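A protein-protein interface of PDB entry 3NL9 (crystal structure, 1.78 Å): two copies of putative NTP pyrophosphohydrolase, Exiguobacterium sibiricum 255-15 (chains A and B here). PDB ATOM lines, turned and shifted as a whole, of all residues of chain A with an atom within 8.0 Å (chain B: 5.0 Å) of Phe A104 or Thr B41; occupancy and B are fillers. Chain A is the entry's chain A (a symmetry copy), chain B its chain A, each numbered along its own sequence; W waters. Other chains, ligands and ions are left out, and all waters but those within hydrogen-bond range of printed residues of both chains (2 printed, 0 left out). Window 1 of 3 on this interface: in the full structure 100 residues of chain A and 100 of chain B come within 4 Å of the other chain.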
ATOM      1  N   THR A  41       2.255   4.145  33.915  1.00  0.00           N
ATOM      2  CA  THR A  41       3.003   3.144  33.138  1.00  0.00           C
ATOM      3  C   THR A  41       4.220   3.824  32.513  1.00  0.00           C
ATOM      4  O   THR A  41       5.352   3.322  32.610  1.00  0.00           O
ATOM      5  CB  THR A  41       2.092   2.465  32.061  1.00  0.00           C
ATOM      6  OG1 THR A  41       0.889   1.959  32.684  1.00  0.00           O
ATOM      7  CG2 THR A  41       2.810   1.330  31.337  1.00  0.00           C
ATOM      8  N   ALA A  42       3.998   4.975  31.885  1.00  0.00           N
ATOM      9  CA  ALA A  42       5.076   5.713  31.228  1.00  0.00           C
ATOM     10  C   ALA A  42       6.076   6.309  32.241  1.00  0.00           C
ATOM     11  O   ALA A  42       7.230   6.486  31.911  1.00  0.00           O
ATOM     12  CB  ALA A  42       4.494   6.846  30.339  1.00  0.00           C
ATOM     13  N   ALA A  45       8.101   3.034  32.416  1.00  0.00           N
ATOM     14  CA  ALA A  45       8.645   2.503  31.135  1.00  0.00           C
ATOM     15  C   ALA A  45       9.413   3.559  30.340  1.00  0.00           C
ATOM     16  O   ALA A  45      10.270   3.202  29.519  1.00  0.00           O
ATOM     17  CB  ALA A  45       7.544   1.951  30.263  1.00  0.00           C
ATOM     18  N   VAL A  46       9.094   4.841  30.552  1.00  0.00           N
ATOM     19  CA  VAL A  46       9.787   5.921  29.823  1.00  0.00           C
ATOM     20  C   VAL A  46      10.746   6.678  30.745  1.00  0.00           C
ATOM     21  O   VAL A  46      11.939   6.663  30.515  1.00  0.00           O
ATOM     22  CB  VAL A  46       8.802   6.903  29.140  1.00  0.00           C
ATOM     23  CG1 VAL A  46       9.562   8.010  28.358  1.00  0.00           C
ATOM     24  CG2 VAL A  46       7.832   6.125  28.223  1.00  0.00           C
ATOM     25  N   PHE A  49      13.058   4.439  33.341  1.00  0.00           N
ATOM     26  CA  PHE A  49      13.872   3.596  32.450  1.00  0.00           C
ATOM     27  C   PHE A  49      14.963   4.424  31.718  1.00  0.00           C
ATOM     28  O   PHE A  49      16.146   3.993  31.608  1.00  0.00           O
ATOM     29  CB  PHE A  49      12.937   2.886  31.461  1.00  0.00           C
ATOM     30  CG  PHE A  49      13.629   2.087  30.425  1.00  0.00           C
ATOM     31  CD1 PHE A  49      14.123   0.826  30.721  1.00  0.00           C
ATOM     32  CD2 PHE A  49      13.805   2.593  29.137  1.00  0.00           C
ATOM     33  CE1 PHE A  49      14.775   0.076  29.742  1.00  0.00           C
ATOM     34  CE2 PHE A  49      14.474   1.849  28.157  1.00  0.00           C
ATOM     35  CZ  PHE A  49      14.963   0.606  28.462  1.00  0.00           C
ATOM     36  N   PHE A  67      12.198  11.025  22.600  1.00  0.00           N
ATOM     37  CA  PHE A  67      10.959  10.346  22.990  1.00  0.00           C
ATOM     38  C   PHE A  67       9.760  11.214  22.694  1.00  0.00           C
ATOM     39  O   PHE A  67       8.795  10.745  22.064  1.00  0.00           O
ATOM     40  CB  PHE A  67      10.926   9.950  24.484  1.00  0.00           C
ATOM     41  CG  PHE A  67       9.565   9.462  24.935  1.00  0.00           C
ATOM     42  CD1 PHE A  67       9.159   8.166  24.654  1.00  0.00           C
ATOM     43  CD2 PHE A  67       8.671  10.323  25.548  1.00  0.00           C
ATOM     44  CE1 PHE A  67       7.903   7.719  25.020  1.00  0.00           C
ATOM     45  CE2 PHE A  67       7.388   9.888  25.899  1.00  0.00           C
ATOM     46  CZ  PHE A  67       7.001   8.595  25.615  1.00  0.00           C
ATOM     47  N   ALA A  97      -4.185  -2.542  22.505  1.00  0.00           N
ATOM     48  CA  ALA A  97      -3.046  -1.667  22.840  1.00  0.00           C
ATOM     49  C   ALA A  97      -2.248  -2.215  24.051  1.00  0.00           C
ATOM     50  O   ALA A  97      -1.030  -2.194  24.068  1.00  0.00           O
ATOM     51  CB  ALA A  97      -3.542  -0.276  23.116  1.00  0.00           C
ATOM     52  N   LEU A  98      -2.959  -2.702  25.056  1.00  0.00           N
ATOM     53  CA  LEU A  98      -2.335  -3.214  26.274  1.00  0.00           C
ATOM     54  C   LEU A  98      -1.498  -4.465  25.942  1.00  0.00           C
ATOM     55  O   LEU A  98      -0.412  -4.666  26.498  1.00  0.00           O
ATOM     56  CB  LEU A  98      -3.388  -3.510  27.354  1.00  0.00           C
ATOM     57  CG  LEU A  98      -4.003  -2.294  28.066  1.00  0.00           C
ATOM     58  CD1 LEU A  98      -5.081  -2.739  29.019  1.00  0.00           C
ATOM     59  CD2 LEU A  98      -2.972  -1.406  28.777  1.00  0.00           C
ATOM     60  N   THR A  99      -1.969  -5.268  24.987  1.00  0.00           N
ATOM     61  CA  THR A  99      -1.254  -6.523  24.615  1.00  0.00           C
ATOM     62  C   THR A  99       0.028  -6.191  23.889  1.00  0.00           C
ATOM     63  O   THR A  99       1.075  -6.788  24.181  1.00  0.00           O
ATOM     64  CB  THR A  99      -2.142  -7.485  23.773  1.00  0.00           C
ATOM     65  OG1 THR A  99      -3.346  -7.790  24.507  1.00  0.00           O
ATOM     66  CG2 THR A  99      -1.430  -8.809  23.471  1.00  0.00           C
ATOM     67  N   ASP A 100      -0.029  -5.298  22.895  1.00  0.00           N
ATOM     68  CA  ASP A 100       1.220  -4.861  22.257  1.00  0.00           C
ATOM     69  C   ASP A 100       2.199  -4.200  23.264  1.00  0.00           C
ATOM     70  O   ASP A 100       3.388  -4.427  23.187  1.00  0.00           O
ATOM     71  CB  ASP A 100       0.983  -3.940  21.049  1.00  0.00           C
ATOM     72  CG  ASP A 100       0.408  -4.668  19.813  1.00  0.00           C
ATOM     73  OD1 ASP A 100       0.448  -5.920  19.719  1.00  0.00           O
ATOM     74  OD2 ASP A 100      -0.130  -3.953  18.940  1.00  0.00           O
ATOM     75  N   ALA A 101       1.700  -3.365  24.166  1.00  0.00           N
ATOM     76  CA  ALA A 101       2.542  -2.735  25.183  1.00  0.00           C
ATOM     77  C   ALA A 101       3.277  -3.817  26.018  1.00  0.00           C
ATOM     78  O   ALA A 101       4.497  -3.776  26.188  1.00  0.00           O
ATOM     79  CB  ALA A 101       1.687  -1.800  26.117  1.00  0.00           C
ATOM     80  N   LEU A 102       2.510  -4.799  26.502  1.00  0.00           N
ATOM     81  CA  LEU A 102       3.067  -5.986  27.202  1.00  0.00           C
ATOM     82  C   LEU A 102       4.155  -6.642  26.373  1.00  0.00           C
ATOM     83  O   LEU A 102       5.247  -6.987  26.892  1.00  0.00           O
ATOM     84  CB  LEU A 102       1.949  -6.996  27.530  1.00  0.00           C
ATOM     85  CG  LEU A 102       2.312  -8.347  28.149  1.00  0.00           C
ATOM     86  CD1 LEU A 102       3.079  -8.151  29.475  1.00  0.00           C
ATOM     87  CD2 LEU A 102       1.058  -9.161  28.342  1.00  0.00           C
ATOM     88  N   TYR A 103       3.897  -6.785  25.067  1.00  0.00           N
ATOM     89  CA  TYR A 103       4.855  -7.453  24.154  1.00  0.00           C
ATOM     90  C   TYR A 103       6.187  -6.673  24.088  1.00  0.00           C
ATOM     91  O   TYR A 103       7.300  -7.235  24.101  1.00  0.00           O
ATOM     92  CB  TYR A 103       4.262  -7.569  22.733  1.00  0.00           C
ATOM     93  CG  TYR A 103       4.818  -8.737  21.952  1.00  0.00           C
ATOM     94  CD1 TYR A 103       5.978  -8.613  21.225  1.00  0.00           C
ATOM     95  CD2 TYR A 103       4.185  -9.979  21.967  1.00  0.00           C
ATOM     96  CE1 TYR A 103       6.492  -9.666  20.531  1.00  0.00           C
ATOM     97  CE2 TYR A 103       4.710 -11.063  21.268  1.00  0.00           C
ATOM     98  CZ  TYR A 103       5.859 -10.885  20.536  1.00  0.00           C
ATOM     99  OH  TYR A 103       6.432 -11.874  19.811  1.00  0.00           O
ATOM    100  N   PHE A 104       6.070  -5.372  23.991  1.00  0.00           N
ATOM    101  CA  PHE A 104       7.263  -4.495  23.932  1.00  0.00           C
ATOM    102  C   PHE A 104       8.058  -4.479  25.247  1.00  0.00           C
ATOM    103  O   PHE A 104       9.262  -4.429  25.243  1.00  0.00           O
ATOM    104  CB  PHE A 104       6.859  -3.067  23.533  1.00  0.00           C
ATOM    105  CG  PHE A 104       6.637  -2.891  22.021  1.00  0.00           C
ATOM    106  CD1 PHE A 104       7.685  -3.110  21.143  1.00  0.00           C
ATOM    107  CD2 PHE A 104       5.414  -2.488  21.514  1.00  0.00           C
ATOM    108  CE1 PHE A 104       7.532  -2.924  19.781  1.00  0.00           C
ATOM    109  CE2 PHE A 104       5.246  -2.286  20.147  1.00  0.00           C
ATOM    110  CZ  PHE A 104       6.306  -2.527  19.276  1.00  0.00           C
ATOM    111  N   ILE A 105       7.349  -4.486  26.364  1.00  0.00           N
ATOM    112  CA  ILE A 105       7.979  -4.568  27.672  1.00  0.00           C
ATOM    113  C   ILE A 105       8.786  -5.861  27.715  1.00  0.00           C
ATOM    114  O   ILE A 105       9.984  -5.858  28.006  1.00  0.00           O
ATOM    115  CB  ILE A 105       6.920  -4.512  28.771  1.00  0.00           C
ATOM    116  CG1 ILE A 105       6.515  -3.048  29.003  1.00  0.00           C
ATOM    117  CG2 ILE A 105       7.440  -5.150  30.096  1.00  0.00           C
ATOM    118  CD1 ILE A 105       5.143  -2.884  29.641  1.00  0.00           C
ATOM    119  N   MET A 106       8.148  -6.952  27.317  1.00  0.00           N
ATOM    120  CA  MET A 106       8.800  -8.238  27.332  1.00  0.00           C
ATOM    121  C   MET A 106      10.046  -8.232  26.460  1.00  0.00           C
ATOM    122  O   MET A 106      11.047  -8.789  26.880  1.00  0.00           O
ATOM    123  CB  MET A 106       7.863  -9.404  26.971  1.00  0.00           C
ATOM    124  CG  MET A 106       6.803  -9.689  28.041  1.00  0.00           C
ATOM    125  SD  MET A 106       7.707 -10.519  29.589  1.00  0.00           S
ATOM    126  CE  MET A 106       6.302 -10.815  30.897  1.00  0.00           C
ATOM    127  N   GLY A 107       9.984  -7.566  25.312  1.00  0.00           N
ATOM    128  CA  GLY A 107      11.138  -7.443  24.402  1.00  0.00           C
ATOM    129  C   GLY A 107      12.293  -6.659  24.986  1.00  0.00           C
ATOM    130  O   GLY A 107      13.464  -6.940  24.704  1.00  0.00           O
ATOM    131  N   SER A 108      11.980  -5.663  25.788  1.00  0.00           N
ATOM    132  CA  SER A 108      12.986  -4.960  26.559  1.00  0.00           C
ATOM    133  C   SER A 108      13.669  -5.883  27.594  1.00  0.00           C
ATOM    134  O   SER A 108      14.872  -5.796  27.762  1.00  0.00           O
ATOM    135  CB  SER A 108      12.392  -3.673  27.198  1.00  0.00           C
ATOM    136  OG  SER A 108      11.830  -2.826  26.191  1.00  0.00           O
ATOM    137  N   PHE A 109      12.911  -6.729  28.312  1.00  0.00           N
ATOM    138  CA  PHE A 109      13.549  -7.755  29.120  1.00  0.00           C
ATOM    139  C   PHE A 109      14.468  -8.605  28.256  1.00  0.00           C
ATOM    140  O   PHE A 109      15.608  -8.850  28.648  1.00  0.00           O
ATOM    141  CB  PHE A 109      12.560  -8.649  29.906  1.00  0.00           C
ATOM    142  CG  PHE A 109      11.999  -7.984  31.131  1.00  0.00           C
ATOM    143  CD1 PHE A 109      12.749  -7.918  32.304  1.00  0.00           C
ATOM    144  CD2 PHE A 109      10.766  -7.387  31.109  1.00  0.00           C
ATOM    145  CE1 PHE A 109      12.258  -7.306  33.417  1.00  0.00           C
ATOM    146  CE2 PHE A 109      10.264  -6.762  32.229  1.00  0.00           C
ATOM    147  CZ  PHE A 109      11.013  -6.728  33.388  1.00  0.00           C
ATOM    148  N   VAL A 110      14.002  -9.041  27.081  1.00  0.00           N
ATOM    149  CA  VAL A 110      14.853  -9.890  26.198  1.00  0.00           C
ATOM    150  C   VAL A 110      16.139  -9.132  25.825  1.00  0.00           C
ATOM    151  O   VAL A 110      17.245  -9.707  25.793  1.00  0.00           O
ATOM    152  CB  VAL A 110      14.093 -10.331  24.912  1.00  0.00           C
ATOM    153  CG1 VAL A 110      15.061 -10.870  23.755  1.00  0.00           C
ATOM    154  CG2 VAL A 110      12.966 -11.328  25.275  1.00  0.00           C
ATOM    155  N   GLU A 111      16.015  -7.854  25.514  1.00  0.00           N
ATOM    156  CA  GLU A 111      17.193  -7.102  25.061  1.00  0.00           C
ATOM    157  C   GLU A 111      18.166  -6.876  26.212  1.00  0.00           C
ATOM    158  O   GLU A 111      19.344  -6.787  25.985  1.00  0.00           O
ATOM    159  CB  GLU A 111      16.796  -5.777  24.411  1.00  0.00           C
ATOM    160  CG  GLU A 111      16.035  -5.994  23.139  1.00  0.00           C
ATOM    161  CD  GLU A 111      16.156  -4.888  22.131  1.00  0.00           C
ATOM    162  OE1 GLU A 111      17.144  -4.092  22.156  1.00  0.00           O
ATOM    163  OE2 GLU A 111      15.252  -4.865  21.273  1.00  0.00           O
ATOM    164  N   LYS B  36      14.315   4.016  21.697  1.00  0.00           N
ATOM    165  CA  LYS B  36      13.468   3.382  20.706  1.00  0.00           C
ATOM    166  C   LYS B  36      12.399   2.525  21.391  1.00  0.00           C
ATOM    167  O   LYS B  36      11.224   2.661  21.099  1.00  0.00           O
ATOM    168  CB  LYS B  36      14.301   2.504  19.764  1.00  0.00           C
ATOM    169  CG  LYS B  36      15.248   3.285  18.841  1.00  0.00           C
ATOM    170  CD  LYS B  36      15.916   2.366  17.835  1.00  0.00           C
ATOM    171  CE  LYS B  36      16.790   3.130  16.841  1.00  0.00           C
ATOM    172  NZ  LYS B  36      16.122   4.358  16.301  1.00  0.00           N
ATOM    173  N   ARG B  37      12.838   1.676  22.316  1.00  0.00           N
ATOM    174  CA  ARG B  37      11.953   0.766  23.015  1.00  0.00           C
ATOM    175  C   ARG B  37      10.940   1.495  23.832  1.00  0.00           C
ATOM    176  O   ARG B  37       9.780   1.115  23.825  1.00  0.00           O
ATOM    177  CB  ARG B  37      12.752  -0.238  23.838  1.00  0.00           C
ATOM    178  CG  ARG B  37      13.629  -1.149  22.899  1.00  0.00           C
ATOM    179  CD  ARG B  37      13.822  -2.506  23.428  1.00  0.00           C
ATOM    180  NE  ARG B  37      12.538  -3.182  23.525  1.00  0.00           N
ATOM    181  CZ  ARG B  37      11.949  -3.888  22.559  1.00  0.00           C
ATOM    182  NH1 ARG B  37      12.524  -4.083  21.357  1.00  0.00           N
ATOM    183  NH2 ARG B  37      10.768  -4.410  22.815  1.00  0.00           N
ATOM    184  N   ALA B  38      11.383   2.539  24.541  1.00  0.00           N
ATOM    185  CA  ALA B  38      10.474   3.391  25.316  1.00  0.00           C
ATOM    186  C   ALA B  38       9.394   3.999  24.420  1.00  0.00           C
ATOM    187  O   ALA B  38       8.209   4.000  24.745  1.00  0.00           O
ATOM    188  CB  ALA B  38      11.284   4.489  26.027  1.00  0.00           C
ATOM    189  N   THR B  39       9.823   4.494  23.268  1.00  0.00           N
ATOM    190  CA  THR B  39       8.938   5.095  22.279  1.00  0.00           C
ATOM    191  C   THR B  39       7.917   4.081  21.760  1.00  0.00           C
ATOM    192  O   THR B  39       6.733   4.360  21.806  1.00  0.00           O
ATOM    193  CB  THR B  39       9.752   5.741  21.114  1.00  0.00           C
ATOM    194  OG1 THR B  39      10.680   6.698  21.673  1.00  0.00           O
ATOM    195  CG2 THR B  39       8.802   6.426  20.106  1.00  0.00           C
ATOM    196  N   TRP B  40       8.358   2.896  21.332  1.00  0.00           N
ATOM    197  CA  TRP B  40       7.425   1.883  20.847  1.00  0.00           C
ATOM    198  C   TRP B  40       6.425   1.472  21.905  1.00  0.00           C
ATOM    199  O   TRP B  40       5.239   1.226  21.588  1.00  0.00           O
ATOM    200  CB  TRP B  40       8.153   0.649  20.351  1.00  0.00           C
ATOM    201  CG  TRP B  40       9.078   0.918  19.210  1.00  0.00           C
ATOM    202  CD1 TRP B  40       8.902   1.830  18.220  1.00  0.00           C
ATOM    203  CD2 TRP B  40      10.302   0.227  18.903  1.00  0.00           C
ATOM    204  NE1 TRP B  40       9.947   1.779  17.336  1.00  0.00           N
ATOM    205  CE2 TRP B  40      10.817   0.802  17.720  1.00  0.00           C
ATOM    206  CE3 TRP B  40      11.005  -0.821  19.508  1.00  0.00           C
ATOM    207  CZ2 TRP B  40      12.024   0.385  17.139  1.00  0.00           C
ATOM    208  CZ3 TRP B  40      12.219  -1.240  18.929  1.00  0.00           C
ATOM    209  CH2 TRP B  40      12.706  -0.639  17.759  1.00  0.00           C
ATOM    210  N   THR B  41       6.901   1.356  23.153  1.00  0.00           N
ATOM    211  CA  THR B  41       6.047   0.902  24.262  1.00  0.00           C
ATOM    212  C   THR B  41       4.956   1.946  24.494  1.00  0.00           C
ATOM    213  O   THR B  41       3.763   1.613  24.587  1.00  0.00           O
ATOM    214  CB  THR B  41       6.888   0.632  25.554  1.00  0.00           C
ATOM    215  OG1 THR B  41       7.989  -0.253  25.248  1.00  0.00           O
ATOM    216  CG2 THR B  41       6.043   0.032  26.673  1.00  0.00           C
ATOM    217  N   ALA B  42       5.356   3.212  24.572  1.00  0.00           N
ATOM    218  CA  ALA B  42       4.411   4.303  24.813  1.00  0.00           C
ATOM    219  C   ALA B  42       3.473   4.537  23.612  1.00  0.00           C
ATOM    220  O   ALA B  42       2.365   4.997  23.797  1.00  0.00           O
ATOM    221  CB  ALA B  42       5.173   5.615  25.146  1.00  0.00           C
ATOM    222  N   GLU B  43       3.919   4.248  22.383  1.00  0.00           N
ATOM    223  CA  GLU B  43       3.022   4.371  21.189  1.00  0.00           C
ATOM    224  C   GLU B  43       1.774   3.531  21.421  1.00  0.00           C
ATOM    225  O   GLU B  43       0.639   3.949  21.119  1.00  0.00           O
ATOM    226  CB  GLU B  43       3.734   3.933  19.890  1.00  0.00           C
ATOM    227  CG  GLU B  43       4.669   4.981  19.313  1.00  0.00           C
ATOM    228  CD  GLU B  43       5.613   4.466  18.203  1.00  0.00           C
ATOM    229  OE1 GLU B  43       5.575   3.270  17.841  1.00  0.00           O
ATOM    230  OE2 GLU B  43       6.401   5.278  17.686  1.00  0.00           O
ATOM    231  N   GLU B  44       1.973   2.376  22.043  1.00  0.00           N
ATOM    232  CA  GLU B  44       0.854   1.489  22.366  1.00  0.00           C
ATOM    233  C   GLU B  44       0.218   1.803  23.731  1.00  0.00           C
ATOM    234  O   GLU B  44      -0.980   2.074  23.798  1.00  0.00           O
ATOM    235  CB  GLU B  44       1.312   0.033  22.244  1.00  0.00           C
ATOM    236  CG  GLU B  44       1.706  -0.323  20.812  1.00  0.00           C
ATOM    237  CD  GLU B  44       0.498  -0.479  19.879  1.00  0.00           C
ATOM    238  OE1 GLU B  44      -0.664  -0.583  20.361  1.00  0.00           O
ATOM    239  OE2 GLU B  44       0.704  -0.461  18.652  1.00  0.00           O
ATOM    240  N   ALA B  45       1.008   1.821  24.800  1.00  0.00           N
ATOM    241  CA  ALA B  45       0.436   1.975  26.167  1.00  0.00           C
ATOM    242  C   ALA B  45      -0.153   3.366  26.405  1.00  0.00           C
ATOM    243  O   ALA B  45      -1.025   3.519  27.272  1.00  0.00           O
ATOM    244  CB  ALA B  45       1.477   1.704  27.225  1.00  0.00           C
ATOM    245  N   VAL B  46       0.334   4.373  25.672  1.00  0.00           N
ATOM    246  CA  VAL B  46      -0.179   5.746  25.843  1.00  0.00           C
ATOM    247  C   VAL B  46      -1.052   6.158  24.655  1.00  0.00           C
ATOM    248  O   VAL B  46      -2.227   6.409  24.831  1.00  0.00           O
ATOM    249  CB  VAL B  46       0.954   6.779  26.067  1.00  0.00           C
ATOM    250  CG1 VAL B  46       0.380   8.209  26.272  1.00  0.00           C
ATOM    251  CG2 VAL B  46       1.835   6.346  27.260  1.00  0.00           C
HETATM  252  O   HOH W   1      -0.966  -2.397  16.925  1.00  0.00           O
HETATM  253  O   HOH W   2       9.909  -1.299  27.062  1.00  0.00           O
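Water W2 lies within hydrogen-bond range of the side-chain hydroxyl (OG) of Ser A108 and the side-chain hydroxyl (OG1) of Thr B41.
Water W1 lies within hydrogen-bond range of the side-chain carboxylate of Asp A100 (2.7 Å) and the side-chain carboxylate of Glu B44 (3.1 Å).
Among the printed residues, merely in contact across the chains: Ala A45 with Ala B38 (3.9 Å), Phe A67 with Ala B38 (3.7 Å), Phe A67 with Thr B39 (3.7 Å), Phe A67 with Ala B42 (3.4 Å), Ala A97 with Glu B44 (3.5 Å), Asp A100 with Glu B44 (3.6 Å), Ala A101 with Glu B44 (3.9 Å), Ala A101 with Ala B45 (3.7 Å), Phe A104 with Trp B40 (3.7 Å), Phe A104 with Thr B41 (3.5 Å), Ile A105 with Thr B41 (3.9 Å) and Gly A107 with Arg B37 (3.4 Å).
Positions printed for both chains: 41, 42, 45 and 46.
The backbone carbonyl oxygen (O) of Arg B37 sits at hydrogen-bond distance from the side-chain hydroxyl (OG1) of Thr B41 (2.7 Å).
The backbone carbonyl oxygen (O) of Phe A104 is in hydrogen-bond range of the side-chain hydroxyl (OG) of Ser A108.
O of Phe A104 lies within hydrogen-bond range of NH2 of Arg B37, 2.9 Å away.
The guanidinium group of Arg B37 sits at hydrogen-bond distance from the side-chain hydroxyl of Ser A108 (2.8 Å).
The guanidinium group (NH1) of Arg B37 lies within salt-bridge range of the side-chain carboxylate (OE2) of Glu A111, at 2.8 Å.
Of the printed residues of chain A, Thr B41 touches Phe A104 (3.5 Å) and Ile A105 (3.9 Å).
Ala B42 touches one residue of chain A.
Of the printed residues of chain A, Arg B37 touches Phe A104 (2.9 Å), Gly A107 (3.4 Å), Ser A108 (2.8 Å) and Glu A111 (2.8 Å).
Printed residues of chain B within 4 Å of Glu A111: Arg B37 (2.8 Å).
Printed residues of chain B within 4 Å of Ala A45: Ala B38.
Met A106 touches none of the printed residues of chain B.
Thr A41 touches none of the printed residues of chain B.
Of the 11 printed residues of chain B, 8 touch a printed residue of chain A.
Printed residues of chain B that touch a printed residue of chain A: Arg B37, Ala B38, Thr B39, Trp B40, Thr B41, Ala B42, Glu B44 and Ala B45.
Printed residues of chain A that touch a printed residue of chain B: Ala A45, Phe A67, Ala A97, Asp A100, Ala A101, Phe A104, Ile A105, Gly A107, Ser A108 and Glu A111.
Among the printed residues, Asp or Glu carboxylates within 4 Å of a Lys or Arg side-chain nitrogen of the other chain: Glu A111 with Arg B37.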
